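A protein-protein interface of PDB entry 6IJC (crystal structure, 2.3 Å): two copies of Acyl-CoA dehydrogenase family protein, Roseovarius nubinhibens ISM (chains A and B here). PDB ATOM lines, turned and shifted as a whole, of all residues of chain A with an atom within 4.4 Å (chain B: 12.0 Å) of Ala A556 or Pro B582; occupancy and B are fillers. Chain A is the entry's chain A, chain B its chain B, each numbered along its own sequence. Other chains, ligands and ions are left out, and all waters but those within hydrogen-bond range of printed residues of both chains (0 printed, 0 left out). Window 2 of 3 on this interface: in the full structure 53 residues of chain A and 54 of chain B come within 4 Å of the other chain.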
ATOM      1  N   ARG A 345      22.047  35.219 -19.280  1.00  0.00           N
ATOM      2  CA  ARG A 345      21.502  34.623 -20.466  1.00  0.00           C
ATOM      3  C   ARG A 345      20.969  33.232 -20.201  1.00  0.00           C
ATOM      4  O   ARG A 345      19.936  32.909 -20.681  1.00  0.00           O
ATOM      5  CB  ARG A 345      22.458  34.635 -21.646  1.00  0.00           C
ATOM      6  CG  ARG A 345      21.832  34.100 -22.916  1.00  0.00           C
ATOM      7  CD  ARG A 345      22.642  34.343 -24.165  1.00  0.00           C
ATOM      8  NE  ARG A 345      22.312  35.620 -24.781  1.00  0.00           N
ATOM      9  CZ  ARG A 345      22.803  36.771 -24.356  1.00  0.00           C
ATOM     10  NH1 ARG A 345      22.492  37.923 -24.938  1.00  0.00           N
ATOM     11  NH2 ARG A 345      23.625  36.756 -23.334  1.00  0.00           N
ATOM     12  N   LEU A 349      17.057  32.057 -20.407  1.00  0.00           N
ATOM     13  CA  LEU A 349      16.720  30.963 -21.310  1.00  0.00           C
ATOM     14  C   LEU A 349      16.077  29.789 -20.585  1.00  0.00           C
ATOM     15  O   LEU A 349      15.257  29.085 -21.183  1.00  0.00           O
ATOM     16  CB  LEU A 349      17.960  30.491 -22.068  1.00  0.00           C
ATOM     17  CG  LEU A 349      18.272  31.304 -23.327  1.00  0.00           C
ATOM     18  CD1 LEU A 349      19.671  30.981 -23.845  1.00  0.00           C
ATOM     19  CD2 LEU A 349      17.196  31.082 -24.423  1.00  0.00           C
ATOM     20  N   GLU A 552      13.040  30.974 -36.024  1.00  0.00           N
ATOM     21  CA  GLU A 552      14.431  30.647 -35.724  1.00  0.00           C
ATOM     22  C   GLU A 552      14.684  30.709 -34.221  1.00  0.00           C
ATOM     23  O   GLU A 552      15.446  29.897 -33.684  1.00  0.00           O
ATOM     24  CB  GLU A 552      15.387  31.590 -36.463  1.00  0.00           C
ATOM     25  CG  GLU A 552      15.244  31.643 -37.984  1.00  0.00           C
ATOM     26  CD  GLU A 552      16.105  30.588 -38.707  1.00  0.00           C
ATOM     27  OE1 GLU A 552      16.490  29.564 -38.093  1.00  0.00           O
ATOM     28  OE2 GLU A 552      16.438  30.784 -39.901  1.00  0.00           O
ATOM     29  N   THR A 553      14.051  31.656 -33.524  1.00  0.00           N
ATOM     30  CA  THR A 553      14.121  31.667 -32.061  1.00  0.00           C
ATOM     31  C   THR A 553      13.448  30.427 -31.465  1.00  0.00           C
ATOM     32  O   THR A 553      14.018  29.778 -30.575  1.00  0.00           O
ATOM     33  CB  THR A 553      13.498  32.959 -31.512  1.00  0.00           C
ATOM     34  OG1 THR A 553      14.080  34.087 -32.187  1.00  0.00           O
ATOM     35  CG2 THR A 553      13.751  33.104 -30.013  1.00  0.00           C
ATOM     36  N   LYS A 554      12.257  30.059 -31.973  1.00  0.00           N
ATOM     37  CA  LYS A 554      11.609  28.811 -31.559  1.00  0.00           C
ATOM     38  C   LYS A 554      12.563  27.633 -31.637  1.00  0.00           C
ATOM     39  O   LYS A 554      12.619  26.812 -30.711  1.00  0.00           O
ATOM     40  CB  LYS A 554      10.371  28.512 -32.415  1.00  0.00           C
ATOM     41  CG  LYS A 554       9.091  29.162 -31.935  1.00  0.00           C
ATOM     42  CD  LYS A 554       8.738  28.755 -30.520  1.00  0.00           C
ATOM     43  CE  LYS A 554       7.514  29.538 -30.037  1.00  0.00           C
ATOM     44  NZ  LYS A 554       7.102  29.164 -28.646  1.00  0.00           N
ATOM     45  N   LEU A 555      13.332  27.540 -32.732  1.00  0.00           N
ATOM     46  CA  LEU A 555      14.245  26.412 -32.900  1.00  0.00           C
ATOM     47  C   LEU A 555      15.356  26.433 -31.859  1.00  0.00           C
ATOM     48  O   LEU A 555      15.697  25.390 -31.291  1.00  0.00           O
ATOM     49  CB  LEU A 555      14.822  26.415 -34.318  1.00  0.00           C
ATOM     50  CG  LEU A 555      13.786  25.880 -35.322  1.00  0.00           C
ATOM     51  CD1 LEU A 555      14.193  26.110 -36.757  1.00  0.00           C
ATOM     52  CD2 LEU A 555      13.546  24.405 -35.086  1.00  0.00           C
ATOM     53  N   ALA A 556      15.941  27.605 -31.608  1.00  0.00           N
ATOM     54  CA  ALA A 556      17.022  27.703 -30.631  1.00  0.00           C
ATOM     55  C   ALA A 556      16.515  27.447 -29.216  1.00  0.00           C
ATOM     56  O   ALA A 556      17.204  26.821 -28.409  1.00  0.00           O
ATOM     57  CB  ALA A 556      17.685  29.080 -30.716  1.00  0.00           C
ATOM     58  N   THR A 557      15.318  27.939 -28.893  1.00  0.00           N
ATOM     59  CA  THR A 557      14.736  27.649 -27.586  1.00  0.00           C
ATOM     60  C   THR A 557      14.463  26.152 -27.425  1.00  0.00           C
ATOM     61  O   THR A 557      14.710  25.583 -26.355  1.00  0.00           O
ATOM     62  CB  THR A 557      13.461  28.470 -27.391  1.00  0.00           C
ATOM     63  OG1 THR A 557      13.686  29.814 -27.858  1.00  0.00           O
ATOM     64  CG2 THR A 557      13.088  28.517 -25.922  1.00  0.00           C
ATOM     65  N   ALA A 558      13.996  25.485 -28.488  1.00  0.00           N
ATOM     66  CA  ALA A 558      13.780  24.039 -28.403  1.00  0.00           C
ATOM     67  C   ALA A 558      15.085  23.298 -28.129  1.00  0.00           C
ATOM     68  O   ALA A 558      15.129  22.401 -27.281  1.00  0.00           O
ATOM     69  CB  ALA A 558      13.128  23.507 -29.683  1.00  0.00           C
ATOM     70  N   ARG A 559      16.159  23.646 -28.851  1.00  0.00           N
ATOM     71  CA  ARG A 559      17.452  23.012 -28.588  1.00  0.00           C
ATOM     72  C   ARG A 559      17.859  23.206 -27.137  1.00  0.00           C
ATOM     73  O   ARG A 559      18.428  22.302 -26.515  1.00  0.00           O
ATOM     74  CB  ARG A 559      18.549  23.589 -29.492  1.00  0.00           C
ATOM     75  CG  ARG A 559      18.289  23.518 -30.978  1.00  0.00           C
ATOM     76  CD  ARG A 559      19.358  24.296 -31.823  1.00  0.00           C
ATOM     77  NE  ARG A 559      18.923  24.284 -33.219  1.00  0.00           N
ATOM     78  CZ  ARG A 559      18.501  25.351 -33.893  1.00  0.00           C
ATOM     79  NH1 ARG A 559      18.520  26.548 -33.329  1.00  0.00           N
ATOM     80  NH2 ARG A 559      18.082  25.226 -35.148  1.00  0.00           N
ATOM     81  N   PHE A 560      17.610  24.398 -26.591  1.00  0.00           N
ATOM     82  CA  PHE A 560      17.966  24.641 -25.202  1.00  0.00           C
ATOM     83  C   PHE A 560      17.193  23.711 -24.278  1.00  0.00           C
ATOM     84  O   PHE A 560      17.777  23.068 -23.396  1.00  0.00           O
ATOM     85  CB  PHE A 560      17.706  26.098 -24.838  1.00  0.00           C
ATOM     86  CG  PHE A 560      18.107  26.449 -23.436  1.00  0.00           C
ATOM     87  CD1 PHE A 560      17.227  26.270 -22.385  1.00  0.00           C
ATOM     88  CD2 PHE A 560      19.353  26.987 -23.180  1.00  0.00           C
ATOM     89  CE1 PHE A 560      17.577  26.601 -21.096  1.00  0.00           C
ATOM     90  CE2 PHE A 560      19.729  27.324 -21.888  1.00  0.00           C
ATOM     91  CZ  PHE A 560      18.837  27.129 -20.839  1.00  0.00           C
ATOM     92  N   PHE B 498      35.789  20.467 -19.268  1.00  0.00           N
ATOM     93  CA  PHE B 498      35.048  21.413 -20.099  1.00  0.00           C
ATOM     94  C   PHE B 498      35.574  22.827 -19.918  1.00  0.00           C
ATOM     95  O   PHE B 498      35.695  23.574 -20.892  1.00  0.00           O
ATOM     96  CB  PHE B 498      33.551  21.397 -19.779  1.00  0.00           C
ATOM     97  CG  PHE B 498      32.723  22.334 -20.652  1.00  0.00           C
ATOM     98  CD1 PHE B 498      32.289  21.932 -21.902  1.00  0.00           C
ATOM     99  CD2 PHE B 498      32.368  23.610 -20.207  1.00  0.00           C
ATOM    100  CE1 PHE B 498      31.523  22.780 -22.697  1.00  0.00           C
ATOM    101  CE2 PHE B 498      31.603  24.463 -20.998  1.00  0.00           C
ATOM    102  CZ  PHE B 498      31.185  24.049 -22.243  1.00  0.00           C
ATOM    103  N   ASN B 506      36.313  29.473 -25.996  1.00  0.00           N
ATOM    104  CA  ASN B 506      34.929  29.916 -26.035  1.00  0.00           C
ATOM    105  C   ASN B 506      34.474  30.236 -24.621  1.00  0.00           C
ATOM    106  O   ASN B 506      33.678  29.486 -24.045  1.00  0.00           O
ATOM    107  CB  ASN B 506      34.033  28.846 -26.657  1.00  0.00           C
ATOM    108  CG  ASN B 506      32.604  29.320 -26.845  1.00  0.00           C
ATOM    109  OD1 ASN B 506      32.267  30.472 -26.540  1.00  0.00           O
ATOM    110  ND2 ASN B 506      31.750  28.428 -27.351  1.00  0.00           N
ATOM    111  N   ASN B 508      32.354  32.210 -23.340  1.00  0.00           N
ATOM    112  CA  ASN B 508      30.914  32.325 -23.133  1.00  0.00           C
ATOM    113  C   ASN B 508      30.297  30.971 -22.793  1.00  0.00           C
ATOM    114  O   ASN B 508      29.405  30.886 -21.941  1.00  0.00           O
ATOM    115  CB  ASN B 508      30.254  32.930 -24.373  1.00  0.00           C
ATOM    116  CG  ASN B 508      30.436  34.436 -24.454  1.00  0.00           C
ATOM    117  OD1 ASN B 508      31.236  35.015 -23.723  1.00  0.00           O
ATOM    118  ND2 ASN B 508      29.694  35.076 -25.350  1.00  0.00           N
ATOM    119  N   ALA B 509      30.769  29.901 -23.444  1.00  0.00           N
ATOM    120  CA  ALA B 509      30.329  28.551 -23.100  1.00  0.00           C
ATOM    121  C   ALA B 509      30.786  28.158 -21.703  1.00  0.00           C
ATOM    122  O   ALA B 509      30.014  27.581 -20.927  1.00  0.00           O
ATOM    123  CB  ALA B 509      30.850  27.546 -24.128  1.00  0.00           C
ATOM    124  N   ALA B 510      32.039  28.450 -21.363  1.00  0.00           N
ATOM    125  CA  ALA B 510      32.505  28.175 -20.008  1.00  0.00           C
ATOM    126  C   ALA B 510      31.639  28.892 -18.973  1.00  0.00           C
ATOM    127  O   ALA B 510      31.106  28.267 -18.048  1.00  0.00           O
ATOM    128  CB  ALA B 510      33.974  28.576 -19.861  1.00  0.00           C
ATOM    129  N   LEU B 511      31.466  30.204 -19.121  1.00  0.00           N
ATOM    130  CA  LEU B 511      30.787  30.945 -18.070  1.00  0.00           C
ATOM    131  C   LEU B 511      29.293  30.624 -17.988  1.00  0.00           C
ATOM    132  O   LEU B 511      28.703  30.749 -16.909  1.00  0.00           O
ATOM    133  CB  LEU B 511      31.023  32.438 -18.269  1.00  0.00           C
ATOM    134  CG  LEU B 511      32.471  32.885 -18.033  1.00  0.00           C
ATOM    135  CD1 LEU B 511      32.485  34.356 -17.723  1.00  0.00           C
ATOM    136  CD2 LEU B 511      33.147  32.113 -16.900  1.00  0.00           C
ATOM    137  N   ALA B 512      28.680  30.195 -19.088  1.00  0.00           N
ATOM    138  CA  ALA B 512      27.273  29.815 -19.052  1.00  0.00           C
ATOM    139  C   ALA B 512      27.028  28.612 -18.134  1.00  0.00           C
ATOM    140  O   ALA B 512      25.979  28.537 -17.487  1.00  0.00           O
ATOM    141  CB  ALA B 512      26.778  29.536 -20.475  1.00  0.00           C
ATOM    142  N   GLY B 513      27.984  27.681 -18.042  1.00  0.00           N
ATOM    143  CA  GLY B 513      27.902  26.544 -17.155  1.00  0.00           C
ATOM    144  C   GLY B 513      28.311  26.787 -15.715  1.00  0.00           C
ATOM    145  O   GLY B 513      28.254  25.852 -14.910  1.00  0.00           O
ATOM    146  N   ALA B 574      25.410  17.562 -17.482  1.00  0.00           N
ATOM    147  CA  ALA B 574      24.795  17.664 -18.808  1.00  0.00           C
ATOM    148  C   ALA B 574      24.560  19.118 -19.189  1.00  0.00           C
ATOM    149  O   ALA B 574      24.766  19.509 -20.343  1.00  0.00           O
ATOM    150  CB  ALA B 574      23.480  16.890 -18.855  1.00  0.00           C
ATOM    151  N   ARG B 575      24.152  19.943 -18.220  1.00  0.00           N
ATOM    152  CA  ARG B 575      23.933  21.354 -18.501  1.00  0.00           C
ATOM    153  C   ARG B 575      25.248  22.087 -18.769  1.00  0.00           C
ATOM    154  O   ARG B 575      25.252  23.099 -19.477  1.00  0.00           O
ATOM    155  CB  ARG B 575      23.163  21.993 -17.344  1.00  0.00           C
ATOM    156  CG  ARG B 575      21.674  21.659 -17.344  1.00  0.00           C
ATOM    157  CD  ARG B 575      20.941  22.188 -16.091  1.00  0.00           C
ATOM    158  NE  ARG B 575      21.055  23.650 -15.911  1.00  0.00           N
ATOM    159  CZ  ARG B 575      20.210  24.566 -16.398  1.00  0.00           C
ATOM    160  NH1 ARG B 575      19.163  24.206 -17.140  1.00  0.00           N
ATOM    161  NH2 ARG B 575      20.419  25.858 -16.146  1.00  0.00           N
ATOM    162  N   ILE B 576      26.362  21.592 -18.228  1.00  0.00           N
ATOM    163  CA  ILE B 576      27.670  22.191 -18.467  1.00  0.00           C
ATOM    164  C   ILE B 576      28.194  21.811 -19.846  1.00  0.00           C
ATOM    165  O   ILE B 576      28.666  22.665 -20.604  1.00  0.00           O
ATOM    166  CB  ILE B 576      28.664  21.767 -17.365  1.00  0.00           C
ATOM    167  CG1 ILE B 576      28.361  22.455 -16.034  1.00  0.00           C
ATOM    168  CG2 ILE B 576      30.104  22.050 -17.798  1.00  0.00           C
ATOM    169  CD1 ILE B 576      29.124  21.837 -14.854  1.00  0.00           C
ATOM    170  N   GLU B 577      28.144  20.515 -20.179  1.00  0.00           N
ATOM    171  CA  GLU B 577      28.723  20.011 -21.423  1.00  0.00           C
ATOM    172  C   GLU B 577      27.917  20.411 -22.654  1.00  0.00           C
ATOM    173  O   GLU B 577      28.476  20.448 -23.757  1.00  0.00           O
ATOM    174  CB  GLU B 577      28.871  18.488 -21.353  1.00  0.00           C
ATOM    175  CG  GLU B 577      30.080  18.025 -20.550  1.00  0.00           C
ATOM    176  CD  GLU B 577      30.139  16.509 -20.386  1.00  0.00           C
ATOM    177  OE1 GLU B 577      29.085  15.842 -20.517  1.00  0.00           O
ATOM    178  OE2 GLU B 577      31.245  15.983 -20.112  1.00  0.00           O
ATOM    179  N   SER B 578      26.625  20.695 -22.508  1.00  0.00           N
ATOM    180  CA  SER B 578      25.972  21.552 -23.485  1.00  0.00           C
ATOM    181  C   SER B 578      26.738  22.869 -23.524  1.00  0.00           C
ATOM    182  O   SER B 578      27.095  23.427 -22.483  1.00  0.00           O
ATOM    183  CB  SER B 578      24.510  21.785 -23.107  1.00  0.00           C
ATOM    184  OG  SER B 578      24.358  22.926 -22.267  1.00  0.00           O
ATOM    185  N   GLY B 579      27.039  23.356 -24.717  1.00  0.00           N
ATOM    186  CA  GLY B 579      28.004  24.443 -24.779  1.00  0.00           C
ATOM    187  C   GLY B 579      27.465  25.819 -24.448  1.00  0.00           C
ATOM    188  O   GLY B 579      26.705  26.002 -23.488  1.00  0.00           O
ATOM    189  N   ALA B 580      27.869  26.807 -25.242  1.00  0.00           N
ATOM    190  CA  ALA B 580      27.308  28.138 -25.103  1.00  0.00           C
ATOM    191  C   ALA B 580      25.853  28.122 -25.557  1.00  0.00           C
ATOM    192  O   ALA B 580      25.470  27.379 -26.469  1.00  0.00           O
ATOM    193  CB  ALA B 580      28.122  29.157 -25.908  1.00  0.00           C
ATOM    194  N   ASP B 581      25.037  28.928 -24.894  1.00  0.00           N
ATOM    195  CA  ASP B 581      23.630  28.999 -25.220  1.00  0.00           C
ATOM    196  C   ASP B 581      23.442  29.700 -26.569  1.00  0.00           C
ATOM    197  O   ASP B 581      24.372  30.324 -27.087  1.00  0.00           O
ATOM    198  CB  ASP B 581      22.889  29.724 -24.098  1.00  0.00           C
ATOM    199  CG  ASP B 581      23.222  29.153 -22.708  1.00  0.00           C
ATOM    200  OD1 ASP B 581      23.451  27.928 -22.610  1.00  0.00           O
ATOM    201  OD2 ASP B 581      23.256  29.918 -21.717  1.00  0.00           O
ATOM    202  N   PRO B 582      22.266  29.568 -27.182  1.00  0.00           N
ATOM    203  CA  PRO B 582      21.951  30.417 -28.340  1.00  0.00           C
ATOM    204  C   PRO B 582      21.965  31.885 -27.941  1.00  0.00           C
ATOM    205  O   PRO B 582      21.650  32.246 -26.806  1.00  0.00           O
ATOM    206  CB  PRO B 582      20.549  29.955 -28.750  1.00  0.00           C
ATOM    207  CG  PRO B 582      20.447  28.547 -28.231  1.00  0.00           C
ATOM    208  CD  PRO B 582      21.223  28.552 -26.940  1.00  0.00           C
ATOM    209  N   VAL B 583      22.342  32.748 -28.880  1.00  0.00           N
ATOM    210  CA  VAL B 583      22.518  34.149 -28.506  1.00  0.00           C
ATOM    211  C   VAL B 583      21.190  34.914 -28.563  1.00  0.00           C
ATOM    212  O   VAL B 583      20.818  35.577 -27.588  1.00  0.00           O
ATOM    213  CB  VAL B 583      23.635  34.795 -29.353  1.00  0.00           C
ATOM    214  CG1 VAL B 583      24.918  33.990 -29.202  1.00  0.00           C
ATOM    215  CG2 VAL B 583      23.255  34.897 -30.821  1.00  0.00           C
ATOM    216  N   MET B 584      20.441  34.811 -29.666  1.00  0.00           N
ATOM    217  CA  MET B 584      19.107  35.444 -29.833  1.00  0.00           C
ATOM    218  C   MET B 584      18.930  36.787 -29.136  1.00  0.00           C
ATOM    219  O   MET B 584      17.808  37.208 -28.853  1.00  0.00           O
ATOM    220  CB  MET B 584      17.993  34.503 -29.352  1.00  0.00           C
ATOM    221  CG  MET B 584      18.178  33.068 -29.783  1.00  0.00           C
ATOM    222  SD  MET B 584      19.196  32.861 -31.287  1.00  0.00           S
ATOM    223  CE  MET B 584      18.176  33.597 -32.585  1.00  0.00           C
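The backbone carbonyl oxygen of Val B583 lies within hydrogen-bond range of the guanidinium group of Arg A345.
Among the printed residues, pairs that only touch across the chains: Arg A345 with Pro B582 (3.5 Å), Leu A349 with Asp B581 (3.5 Å), Leu A349 with Pro B582 (3.8 Å), Ala A556 with Pro B582 (3.6 Å) and Phe A560 with Asp B581 (3.8 Å).
Of the printed residues of chain B, Leu A349 touches Asp B581 and Pro B582. No residue of chain B comes within 4 Å of Thr A553. No residue of chain B comes within 4 Å of Leu A555. Printed residues of chain B within 4 Å of Ala A556: Pro B582. No residue of chain B comes within 4 Å of Thr A557. No residue of chain B comes within 4 Å of Ala A558. No residue of chain B comes within 4 Å of Arg A559. Of chain A, only Arg A345, Leu A349 and Ala A556 come within 4 Å of Pro B582. Printed residues of chain A within 4 Å of Val B583: Arg A345. The nearest residue of chain B that does not touch Ala A556 is Met B584 (4.1 Å). The nearest printed residue of chain B that does not touch Arg A345 is Asp B581 (4.3 Å).
No position is printed for both chains.
Printed residues of chain A that touch a printed residue of chain B: Arg A345, Leu A349, Ala A556 and Phe A560. Of the 19 printed residues of chain B, 3 touch a printed residue of chain A. Hydrophobic or aromatic side chains of chain B within 4 Å of the printed part of chain A: Pro B582. Along chain B the printed residues that touch a printed residue of chain A span positions 581 to 583.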
